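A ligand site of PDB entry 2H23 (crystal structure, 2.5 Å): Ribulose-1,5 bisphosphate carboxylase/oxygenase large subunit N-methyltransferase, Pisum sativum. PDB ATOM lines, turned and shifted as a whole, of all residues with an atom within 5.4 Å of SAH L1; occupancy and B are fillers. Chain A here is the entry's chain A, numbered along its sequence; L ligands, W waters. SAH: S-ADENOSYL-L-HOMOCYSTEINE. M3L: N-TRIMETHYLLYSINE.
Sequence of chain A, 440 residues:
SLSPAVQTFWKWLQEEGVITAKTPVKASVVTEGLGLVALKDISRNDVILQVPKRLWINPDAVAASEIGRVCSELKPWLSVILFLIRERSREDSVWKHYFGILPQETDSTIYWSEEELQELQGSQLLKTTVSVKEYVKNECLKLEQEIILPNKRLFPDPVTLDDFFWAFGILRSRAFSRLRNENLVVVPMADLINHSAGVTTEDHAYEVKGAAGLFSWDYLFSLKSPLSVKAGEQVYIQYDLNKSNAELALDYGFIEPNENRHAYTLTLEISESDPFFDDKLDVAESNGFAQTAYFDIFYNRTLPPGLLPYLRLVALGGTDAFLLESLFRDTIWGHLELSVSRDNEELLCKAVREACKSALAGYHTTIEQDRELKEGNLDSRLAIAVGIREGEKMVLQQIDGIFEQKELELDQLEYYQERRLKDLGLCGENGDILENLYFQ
The backbone carbonyl oxygen (O) of Ser 173 lies close to a sulfur (SD) of SAH L1, at 3.6 Å. SD of SAH L1 lies close to O of Asp 191 (3.6 Å). Merely in contact with SAH L1: Gly 33, Pro 103, Thr 106, Leu 192, Ile 193, Tyr 239, Tyr 252, Gly 253 and Phe 254. Hydrophobic or aromatic side chains that line SAH L1: Leu 34, Pro 103, His 195, Tyr 239, Tyr 252 and Phe 254. Within 4 Å of SAH L1: Glu 32, Gly 33, Leu 34, Pro 103, Thr 106, Ser 173, Arg 174, Asp 191, Leu 192, Ile 193, Asn 194, His 195, Tyr 239, Tyr 252, Gly 253 and Phe 254. The nearest printed residue that does not touch SAH L1 is Asp 107 (4.7 Å).
OD2 of Asp 191 lies within salt-bridge range of NH1 of Arg 174 (2.5 Å). The backbone carbonyl oxygen (O) of Leu 34 is in hydrogen-bond range of the side-chain amide nitrogen (ND2) of Asn 194. ND1 of His 195 sits at hydrogen-bond distance from N of Tyr 239, at 3.0 Å. OH of Tyr 239 lies within hydrogen-bond range of O of Ile 193.
NH2 of Arg 174 is in salt-bridge range of O of SAH L1, at 2.5 Å. N of Leu 34 lies within hydrogen-bond range of OXT of SAH L1 (2.7 Å). The backbone carbonyl oxygen (O) of Leu 34 sits at hydrogen-bond distance from a nitrogen (N) of SAH L1 (2.7 Å). The backbone NH (N) of His 195 sits at hydrogen-bond distance from a nitrogen (N7) of SAH L1 (3.0 Å). The backbone carbonyl oxygen (O) of His 195 lies within hydrogen-bond range of a nitrogen (N6) of SAH L1 (2.8 Å). OD1 of Asn 194 lies within hydrogen-bond range of N of SAH L1, 2.8 Å away. N of SAH L1 is in hydrogen-bond range of O of Glu 32.
Water W1 lies within hydrogen-bond range of an oxygen (O2') of SAH L1 (2.6 Å), the backbone NH of Asp 107 (2.6 Å) and the backbone carbonyl oxygen of Gly 253 (3.2 Å).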
ATOM      1  N   VAL A  30     -16.845 -17.509  -7.170  1.00  0.00           N
ATOM      2  CA  VAL A  30     -17.850 -16.680  -6.529  1.00  0.00           C
ATOM      3  C   VAL A  30     -18.953 -17.515  -5.905  1.00  0.00           C
ATOM      4  O   VAL A  30     -19.034 -18.719  -6.131  1.00  0.00           O
ATOM      5  CB  VAL A  30     -18.465 -15.719  -7.538  1.00  0.00           C
ATOM      6  CG1 VAL A  30     -17.445 -14.690  -7.960  1.00  0.00           C
ATOM      7  CG2 VAL A  30     -18.949 -16.488  -8.753  1.00  0.00           C
ATOM      8  N   GLU A  32     -21.779 -17.843  -6.687  1.00  0.00           N
ATOM      9  CA  GLU A  32     -22.545 -18.482  -7.736  1.00  0.00           C
ATOM     10  C   GLU A  32     -21.763 -19.547  -8.504  1.00  0.00           C
ATOM     11  O   GLU A  32     -22.233 -20.078  -9.505  1.00  0.00           O
ATOM     12  CB  GLU A  32     -23.106 -17.429  -8.695  1.00  0.00           C
ATOM     13  CG  GLU A  32     -22.205 -16.226  -8.875  1.00  0.00           C
ATOM     14  CD  GLU A  32     -22.404 -15.138  -7.828  1.00  0.00           C
ATOM     15  OE1 GLU A  32     -23.438 -14.441  -7.877  1.00  0.00           O
ATOM     16  OE2 GLU A  32     -21.520 -14.962  -6.948  1.00  0.00           O
ATOM     17  N   GLY A  33     -20.570 -19.879  -7.992  1.00  0.00           N
ATOM     18  CA  GLY A  33     -19.746 -20.899  -8.609  1.00  0.00           C
ATOM     19  C   GLY A  33     -18.437 -20.358  -9.146  1.00  0.00           C
ATOM     20  O   GLY A  33     -17.451 -20.236  -8.421  1.00  0.00           O
ATOM     21  N   LEU A  34     -18.440 -20.057 -10.437  1.00  0.00           N
ATOM     22  CA  LEU A  34     -17.295 -19.490 -11.123  1.00  0.00           C
ATOM     23  C   LEU A  34     -17.857 -18.273 -11.827  1.00  0.00           C
ATOM     24  O   LEU A  34     -18.976 -18.331 -12.338  1.00  0.00           O
ATOM     25  CB  LEU A  34     -16.736 -20.460 -12.169  1.00  0.00           C
ATOM     26  CG  LEU A  34     -15.969 -21.651 -11.634  1.00  0.00           C
ATOM     27  CD1 LEU A  34     -15.748 -22.649 -12.758  1.00  0.00           C
ATOM     28  CD2 LEU A  34     -14.645 -21.183 -11.038  1.00  0.00           C
ATOM     29  N   GLY A  35     -17.105 -17.185 -11.862  1.00  0.00           N
ATOM     30  CA  GLY A  35     -17.626 -16.014 -12.521  1.00  0.00           C
ATOM     31  C   GLY A  35     -16.543 -15.105 -13.021  1.00  0.00           C
ATOM     32  O   GLY A  35     -15.351 -15.347 -12.810  1.00  0.00           O
ATOM     33  N   ILE A 101     -13.634 -27.736 -16.273  1.00  0.00           N
ATOM     34  CA  ILE A 101     -14.173 -26.591 -15.588  1.00  0.00           C
ATOM     35  C   ILE A 101     -15.685 -26.723 -15.383  1.00  0.00           C
ATOM     36  O   ILE A 101     -16.208 -26.315 -14.339  1.00  0.00           O
ATOM     37  CB  ILE A 101     -13.805 -25.297 -16.356  1.00  0.00           C
ATOM     38  CG1 ILE A 101     -12.307 -25.075 -16.236  1.00  0.00           C
ATOM     39  CG2 ILE A 101     -14.541 -24.090 -15.795  1.00  0.00           C
ATOM     40  CD1 ILE A 101     -11.807 -25.045 -14.800  1.00  0.00           C
ATOM     41  N   PRO A 103     -19.293 -27.599 -14.258  1.00  0.00           N
ATOM     42  CA  PRO A 103     -19.871 -28.199 -13.057  1.00  0.00           C
ATOM     43  C   PRO A 103     -20.633 -29.468 -13.437  1.00  0.00           C
ATOM     44  O   PRO A 103     -21.472 -29.457 -14.352  1.00  0.00           O
ATOM     45  CB  PRO A 103     -20.808 -27.103 -12.549  1.00  0.00           C
ATOM     46  CG  PRO A 103     -20.089 -25.850 -12.963  1.00  0.00           C
ATOM     47  CD  PRO A 103     -19.699 -26.193 -14.382  1.00  0.00           C
ATOM     48  N   THR A 106     -25.989 -28.684 -11.303  1.00  0.00           N
ATOM     49  CA  THR A 106     -26.461 -27.362 -10.886  1.00  0.00           C
ATOM     50  C   THR A 106     -27.651 -27.582  -9.953  1.00  0.00           C
ATOM     51  O   THR A 106     -27.962 -28.727  -9.603  1.00  0.00           O
ATOM     52  CB  THR A 106     -26.947 -26.477 -12.058  1.00  0.00           C
ATOM     53  OG1 THR A 106     -28.036 -27.129 -12.729  1.00  0.00           O
ATOM     54  CG2 THR A 106     -25.806 -26.199 -13.023  1.00  0.00           C
ATOM     55  N   ASP A 107     -28.319 -26.512  -9.551  1.00  0.00           N
ATOM     56  CA  ASP A 107     -29.451 -26.672  -8.653  1.00  0.00           C
ATOM     57  C   ASP A 107     -30.774 -26.785  -9.377  1.00  0.00           C
ATOM     58  O   ASP A 107     -31.830 -26.752  -8.754  1.00  0.00           O
ATOM     59  CB  ASP A 107     -29.481 -25.557  -7.611  1.00  0.00           C
ATOM     60  CG  ASP A 107     -28.523 -25.819  -6.481  1.00  0.00           C
ATOM     61  OD1 ASP A 107     -28.446 -26.998  -6.058  1.00  0.00           O
ATOM     62  OD2 ASP A 107     -27.842 -24.876  -6.025  1.00  0.00           O
ATOM     63  N   SER A 173     -28.595 -24.229 -19.254  1.00  0.00           N
ATOM     64  CA  SER A 173     -28.012 -23.214 -18.390  1.00  0.00           C
ATOM     65  C   SER A 173     -26.802 -22.526 -18.976  1.00  0.00           C
ATOM     66  O   SER A 173     -26.196 -21.691 -18.314  1.00  0.00           O
ATOM     67  CB  SER A 173     -27.645 -23.843 -17.045  1.00  0.00           C
ATOM     68  OG  SER A 173     -26.633 -24.817 -17.196  1.00  0.00           O
ATOM     69  N   ARG A 174     -26.447 -22.859 -20.210  1.00  0.00           N
ATOM     70  CA  ARG A 174     -25.269 -22.246 -20.835  1.00  0.00           C
ATOM     71  C   ARG A 174     -25.426 -21.841 -22.290  1.00  0.00           C
ATOM     72  O   ARG A 174     -24.474 -21.390 -22.923  1.00  0.00           O
ATOM     73  CB  ARG A 174     -24.079 -23.184 -20.714  1.00  0.00           C
ATOM     74  CG  ARG A 174     -23.727 -23.496 -19.306  1.00  0.00           C
ATOM     75  CD  ARG A 174     -22.532 -24.409 -19.232  1.00  0.00           C
ATOM     76  NE  ARG A 174     -22.116 -24.583 -17.851  1.00  0.00           N
ATOM     77  CZ  ARG A 174     -21.306 -23.757 -17.188  1.00  0.00           C
ATOM     78  NH1 ARG A 174     -20.797 -22.689 -17.793  1.00  0.00           N
ATOM     79  NH2 ARG A 174     -21.030 -23.996 -15.922  1.00  0.00           N
ATOM     80  N   ASP A 191     -19.042 -18.179 -20.976  1.00  0.00           N
ATOM     81  CA  ASP A 191     -19.978 -19.158 -20.441  1.00  0.00           C
ATOM     82  C   ASP A 191     -19.983 -18.965 -18.923  1.00  0.00           C
ATOM     83  O   ASP A 191     -20.918 -19.388 -18.235  1.00  0.00           O
ATOM     84  CB  ASP A 191     -19.457 -20.565 -20.803  1.00  0.00           C
ATOM     85  CG  ASP A 191     -20.568 -21.596 -20.888  1.00  0.00           C
ATOM     86  OD1 ASP A 191     -21.548 -21.373 -21.619  1.00  0.00           O
ATOM     87  OD2 ASP A 191     -20.444 -22.650 -20.223  1.00  0.00           O
ATOM     88  N   LEU A 192     -18.947 -18.299 -18.432  1.00  0.00           N
ATOM     89  CA  LEU A 192     -18.762 -18.060 -17.009  1.00  0.00           C
ATOM     90  C   LEU A 192     -19.378 -16.760 -16.465  1.00  0.00           C
ATOM     91  O   LEU A 192     -19.074 -16.367 -15.336  1.00  0.00           O
ATOM     92  CB  LEU A 192     -17.265 -18.046 -16.702  1.00  0.00           C
ATOM     93  CG  LEU A 192     -16.416 -19.131 -17.362  1.00  0.00           C
ATOM     94  CD1 LEU A 192     -14.953 -18.844 -17.104  1.00  0.00           C
ATOM     95  CD2 LEU A 192     -16.799 -20.494 -16.838  1.00  0.00           C
ATOM     96  N   ILE A 193     -20.223 -16.107 -17.249  1.00  0.00           N
ATOM     97  CA  ILE A 193     -20.863 -14.862 -16.797  1.00  0.00           C
ATOM     98  C   ILE A 193     -22.127 -15.197 -16.016  1.00  0.00           C
ATOM     99  O   ILE A 193     -22.989 -15.942 -16.479  1.00  0.00           O
ATOM    100  CB  ILE A 193     -21.210 -13.961 -18.009  1.00  0.00           C
ATOM    101  CG1 ILE A 193     -21.718 -12.613 -17.535  1.00  0.00           C
ATOM    102  CG2 ILE A 193     -22.264 -14.636 -18.868  1.00  0.00           C
ATOM    103  CD1 ILE A 193     -20.647 -11.740 -16.973  1.00  0.00           C
ATOM    104  N   ASN A 194     -22.240 -14.650 -14.808  1.00  0.00           N
ATOM    105  CA  ASN A 194     -23.413 -14.938 -13.992  1.00  0.00           C
ATOM    106  C   ASN A 194     -24.556 -13.921 -14.125  1.00  0.00           C
ATOM    107  O   ASN A 194     -24.402 -12.867 -14.746  1.00  0.00           O
ATOM    108  CB  ASN A 194     -22.993 -15.080 -12.537  1.00  0.00           C
ATOM    109  CG  ASN A 194     -22.163 -16.323 -12.290  1.00  0.00           C
ATOM    110  OD1 ASN A 194     -22.611 -17.443 -12.563  1.00  0.00           O
ATOM    111  ND2 ASN A 194     -20.964 -16.145 -11.768  1.00  0.00           N
ATOM    112  N   HIS A 195     -25.691 -14.258 -13.514  1.00  0.00           N
ATOM    113  CA  HIS A 195     -26.895 -13.436 -13.545  1.00  0.00           C
ATOM    114  C   HIS A 195     -27.031 -12.515 -12.325  1.00  0.00           C
ATOM    115  O   HIS A 195     -26.696 -12.892 -11.208  1.00  0.00           O
ATOM    116  CB  HIS A 195     -28.129 -14.352 -13.593  1.00  0.00           C
ATOM    117  CG  HIS A 195     -29.418 -13.631 -13.386  1.00  0.00           C
ATOM    118  ND1 HIS A 195     -30.084 -12.977 -14.401  1.00  0.00           N
ATOM    119  CD2 HIS A 195     -30.161 -13.437 -12.261  1.00  0.00           C
ATOM    120  CE1 HIS A 195     -31.183 -12.421 -13.916  1.00  0.00           C
ATOM    121  NE2 HIS A 195     -31.249 -12.686 -12.621  1.00  0.00           N
ATOM    122  N   SER A 196     -27.541 -11.308 -12.546  1.00  0.00           N
ATOM    123  CA  SER A 196     -27.767 -10.360 -11.452  1.00  0.00           C
ATOM    124  C   SER A 196     -28.984  -9.476 -11.694  1.00  0.00           C
ATOM    125  O   SER A 196     -29.186  -8.967 -12.813  1.00  0.00           O
ATOM    126  CB  SER A 196     -26.561  -9.474 -11.211  1.00  0.00           C
ATOM    127  OG  SER A 196     -26.855  -8.590 -10.154  1.00  0.00           O
ATOM    128  N   TYR A 239     -30.116 -12.593 -17.359  1.00  0.00           N
ATOM    129  CA  TYR A 239     -30.429 -13.767 -18.148  1.00  0.00           C
ATOM    130  C   TYR A 239     -31.774 -13.634 -18.879  1.00  0.00           C
ATOM    131  O   TYR A 239     -31.867 -13.936 -20.060  1.00  0.00           O
ATOM    132  CB  TYR A 239     -30.419 -15.040 -17.288  1.00  0.00           C
ATOM    133  CG  TYR A 239     -29.028 -15.521 -16.858  1.00  0.00           C
ATOM    134  CD1 TYR A 239     -28.875 -16.739 -16.195  1.00  0.00           C
ATOM    135  CD2 TYR A 239     -27.882 -14.746 -17.088  1.00  0.00           C
ATOM    136  CE1 TYR A 239     -27.607 -17.186 -15.759  1.00  0.00           C
ATOM    137  CE2 TYR A 239     -26.604 -15.177 -16.660  1.00  0.00           C
ATOM    138  CZ  TYR A 239     -26.481 -16.399 -15.994  1.00  0.00           C
ATOM    139  OH  TYR A 239     -25.235 -16.829 -15.556  1.00  0.00           O
ATOM    140  N   ASP A 251     -34.522 -23.882 -15.577  1.00  0.00           N
ATOM    141  CA  ASP A 251     -33.468 -23.544 -16.539  1.00  0.00           C
ATOM    142  C   ASP A 251     -32.103 -23.450 -15.876  1.00  0.00           C
ATOM    143  O   ASP A 251     -31.124 -24.010 -16.376  1.00  0.00           O
ATOM    144  CB  ASP A 251     -33.783 -22.222 -17.218  1.00  0.00           C
ATOM    145  CG  ASP A 251     -34.669 -22.389 -18.429  1.00  0.00           C
ATOM    146  OD1 ASP A 251     -35.792 -22.928 -18.301  1.00  0.00           O
ATOM    147  OD2 ASP A 251     -34.221 -21.970 -19.517  1.00  0.00           O
ATOM    148  N   TYR A 252     -32.042 -22.734 -14.776  1.00  0.00           N
ATOM    149  CA  TYR A 252     -30.801 -22.581 -14.030  1.00  0.00           C
ATOM    150  C   TYR A 252     -31.119 -23.116 -12.652  1.00  0.00           C
ATOM    151  O   TYR A 252     -32.216 -23.644 -12.436  1.00  0.00           O
ATOM    152  CB  TYR A 252     -30.402 -21.115 -13.945  1.00  0.00           C
ATOM    153  CG  TYR A 252     -30.559 -20.408 -15.262  1.00  0.00           C
ATOM    154  CD1 TYR A 252     -31.697 -19.663 -15.544  1.00  0.00           C
ATOM    155  CD2 TYR A 252     -29.574 -20.532 -16.251  1.00  0.00           C
ATOM    156  CE1 TYR A 252     -31.865 -19.054 -16.784  1.00  0.00           C
ATOM    157  CE2 TYR A 252     -29.735 -19.925 -17.485  1.00  0.00           C
ATOM    158  CZ  TYR A 252     -30.879 -19.192 -17.747  1.00  0.00           C
ATOM    159  OH  TYR A 252     -31.043 -18.613 -18.989  1.00  0.00           O
ATOM    160  N   GLY A 253     -30.195 -22.999 -11.730  1.00  0.00           N
ATOM    161  CA  GLY A 253     -30.486 -23.502 -10.408  1.00  0.00           C
ATOM    162  C   GLY A 253     -30.711 -22.382  -9.415  1.00  0.00           C
ATOM    163  O   GLY A 253     -30.132 -22.434  -8.332  1.00  0.00           O
ATOM    164  N   PHE A 254     -31.541 -21.402  -9.749  1.00  0.00           N
ATOM    165  CA  PHE A 254     -31.755 -20.282  -8.821  1.00  0.00           C
ATOM    166  C   PHE A 254     -33.024 -19.490  -9.083  1.00  0.00           C
ATOM    167  O   PHE A 254     -33.616 -19.565 -10.150  1.00  0.00           O
ATOM    168  CB  PHE A 254     -30.558 -19.304  -8.885  1.00  0.00           C
ATOM    169  CG  PHE A 254     -30.567 -18.399 -10.096  1.00  0.00           C
ATOM    170  CD1 PHE A 254     -31.350 -17.233 -10.114  1.00  0.00           C
ATOM    171  CD2 PHE A 254     -29.808 -18.725 -11.228  1.00  0.00           C
ATOM    172  CE1 PHE A 254     -31.372 -16.406 -11.238  1.00  0.00           C
ATOM    173  CE2 PHE A 254     -29.827 -17.904 -12.359  1.00  0.00           C
ATOM    174  CZ  PHE A 254     -30.605 -16.734 -12.364  1.00  0.00           C
HETATM  175  N   SAH L   1     -21.157 -19.842 -12.206  1.00  0.00           N
HETATM  176  CA  SAH L   1     -21.231 -20.733 -13.361  1.00  0.00           C
HETATM  177  CB  SAH L   1     -21.168 -19.918 -14.684  1.00  0.00           C
HETATM  178  CG  SAH L   1     -22.487 -19.366 -15.163  1.00  0.00           C
HETATM  179  SD  SAH L   1     -23.563 -20.529 -16.087  1.00  0.00           S
HETATM  180  C   SAH L   1     -20.079 -21.801 -13.293  1.00  0.00           C
HETATM  181  O   SAH L   1     -19.877 -22.546 -14.274  1.00  0.00           O
HETATM  182  OXT SAH L   1     -19.376 -21.893 -12.252  1.00  0.00           O
HETATM  183  C5' SAH L   1     -25.076 -20.275 -15.170  1.00  0.00           C
HETATM  184  C4' SAH L   1     -25.213 -21.143 -13.925  1.00  0.00           C
HETATM  185  O4' SAH L   1     -24.428 -20.542 -12.848  1.00  0.00           O
HETATM  186  C3' SAH L   1     -26.625 -21.217 -13.353  1.00  0.00           C
HETATM  187  O3' SAH L   1     -27.417 -22.259 -13.924  1.00  0.00           O
HETATM  188  C2' SAH L   1     -26.394 -21.382 -11.864  1.00  0.00           C
HETATM  189  O2' SAH L   1     -26.176 -22.689 -11.373  1.00  0.00           O
HETATM  190  C1' SAH L   1     -25.232 -20.403 -11.681  1.00  0.00           C
HETATM  191  N9  SAH L   1     -25.678 -18.985 -11.513  1.00  0.00           N
HETATM  192  C8  SAH L   1     -25.634 -17.913 -12.388  1.00  0.00           C
HETATM  193  N7  SAH L   1     -26.119 -16.798 -11.902  1.00  0.00           N
HETATM  194  C5  SAH L   1     -26.516 -17.140 -10.614  1.00  0.00           C
HETATM  195  C6  SAH L   1     -27.121 -16.404  -9.551  1.00  0.00           C
HETATM  196  N6  SAH L   1     -27.445 -15.118  -9.644  1.00  0.00           N
HETATM  197  N1  SAH L   1     -27.388 -17.057  -8.371  1.00  0.00           N
HETATM  198  C2  SAH L   1     -27.070 -18.379  -8.251  1.00  0.00           C
HETATM  199  N3  SAH L   1     -26.494 -19.173  -9.181  1.00  0.00           N
HETATM  200  C4  SAH L   1     -26.240 -18.492 -10.350  1.00  0.00           C
HETATM  201  N   M3L L   2     -30.250 -17.592 -23.317  1.00  0.00           N
HETATM  202  CA  M3L L   2     -30.013 -16.311 -22.657  1.00  0.00           C
HETATM  203  CB  M3L L   2     -28.761 -16.389 -21.782  1.00  0.00           C
HETATM  204  CG  M3L L   2     -28.924 -17.409 -20.647  1.00  0.00           C
HETATM  205  CD  M3L L   2     -27.671 -17.473 -19.769  1.00  0.00           C
HETATM  206  CE  M3L L   2     -26.478 -18.054 -20.521  1.00  0.00           C
HETATM  207  NZ  M3L L   2     -25.256 -18.091 -19.710  1.00  0.00           N
HETATM  208  C   M3L L   2     -29.830 -15.206 -23.698  1.00  0.00           C
HETATM  209  O   M3L L   2     -29.164 -15.387 -24.719  1.00  0.00           O
HETATM  210  OXT M3L L   2     -30.302 -14.112 -23.777  1.00  0.00           O
HETATM  211  CM1 M3L L   2     -25.478 -18.781 -18.433  1.00  0.00           C
HETATM  212  CM2 M3L L   2     -24.231 -18.829 -20.458  1.00  0.00           C
HETATM  213  CM3 M3L L   2     -24.765 -16.728 -19.464  1.00  0.00           C
HETATM  214  O   HOH W   1     -27.688 -23.961  -9.752  1.00  0.00           O
HETATM  215  O   HOH W   2     -23.399 -23.004 -11.577  1.00  0.00           O
HETATM  216  O   HOH W   3     -28.793 -16.740  -5.882  1.00  0.00           O
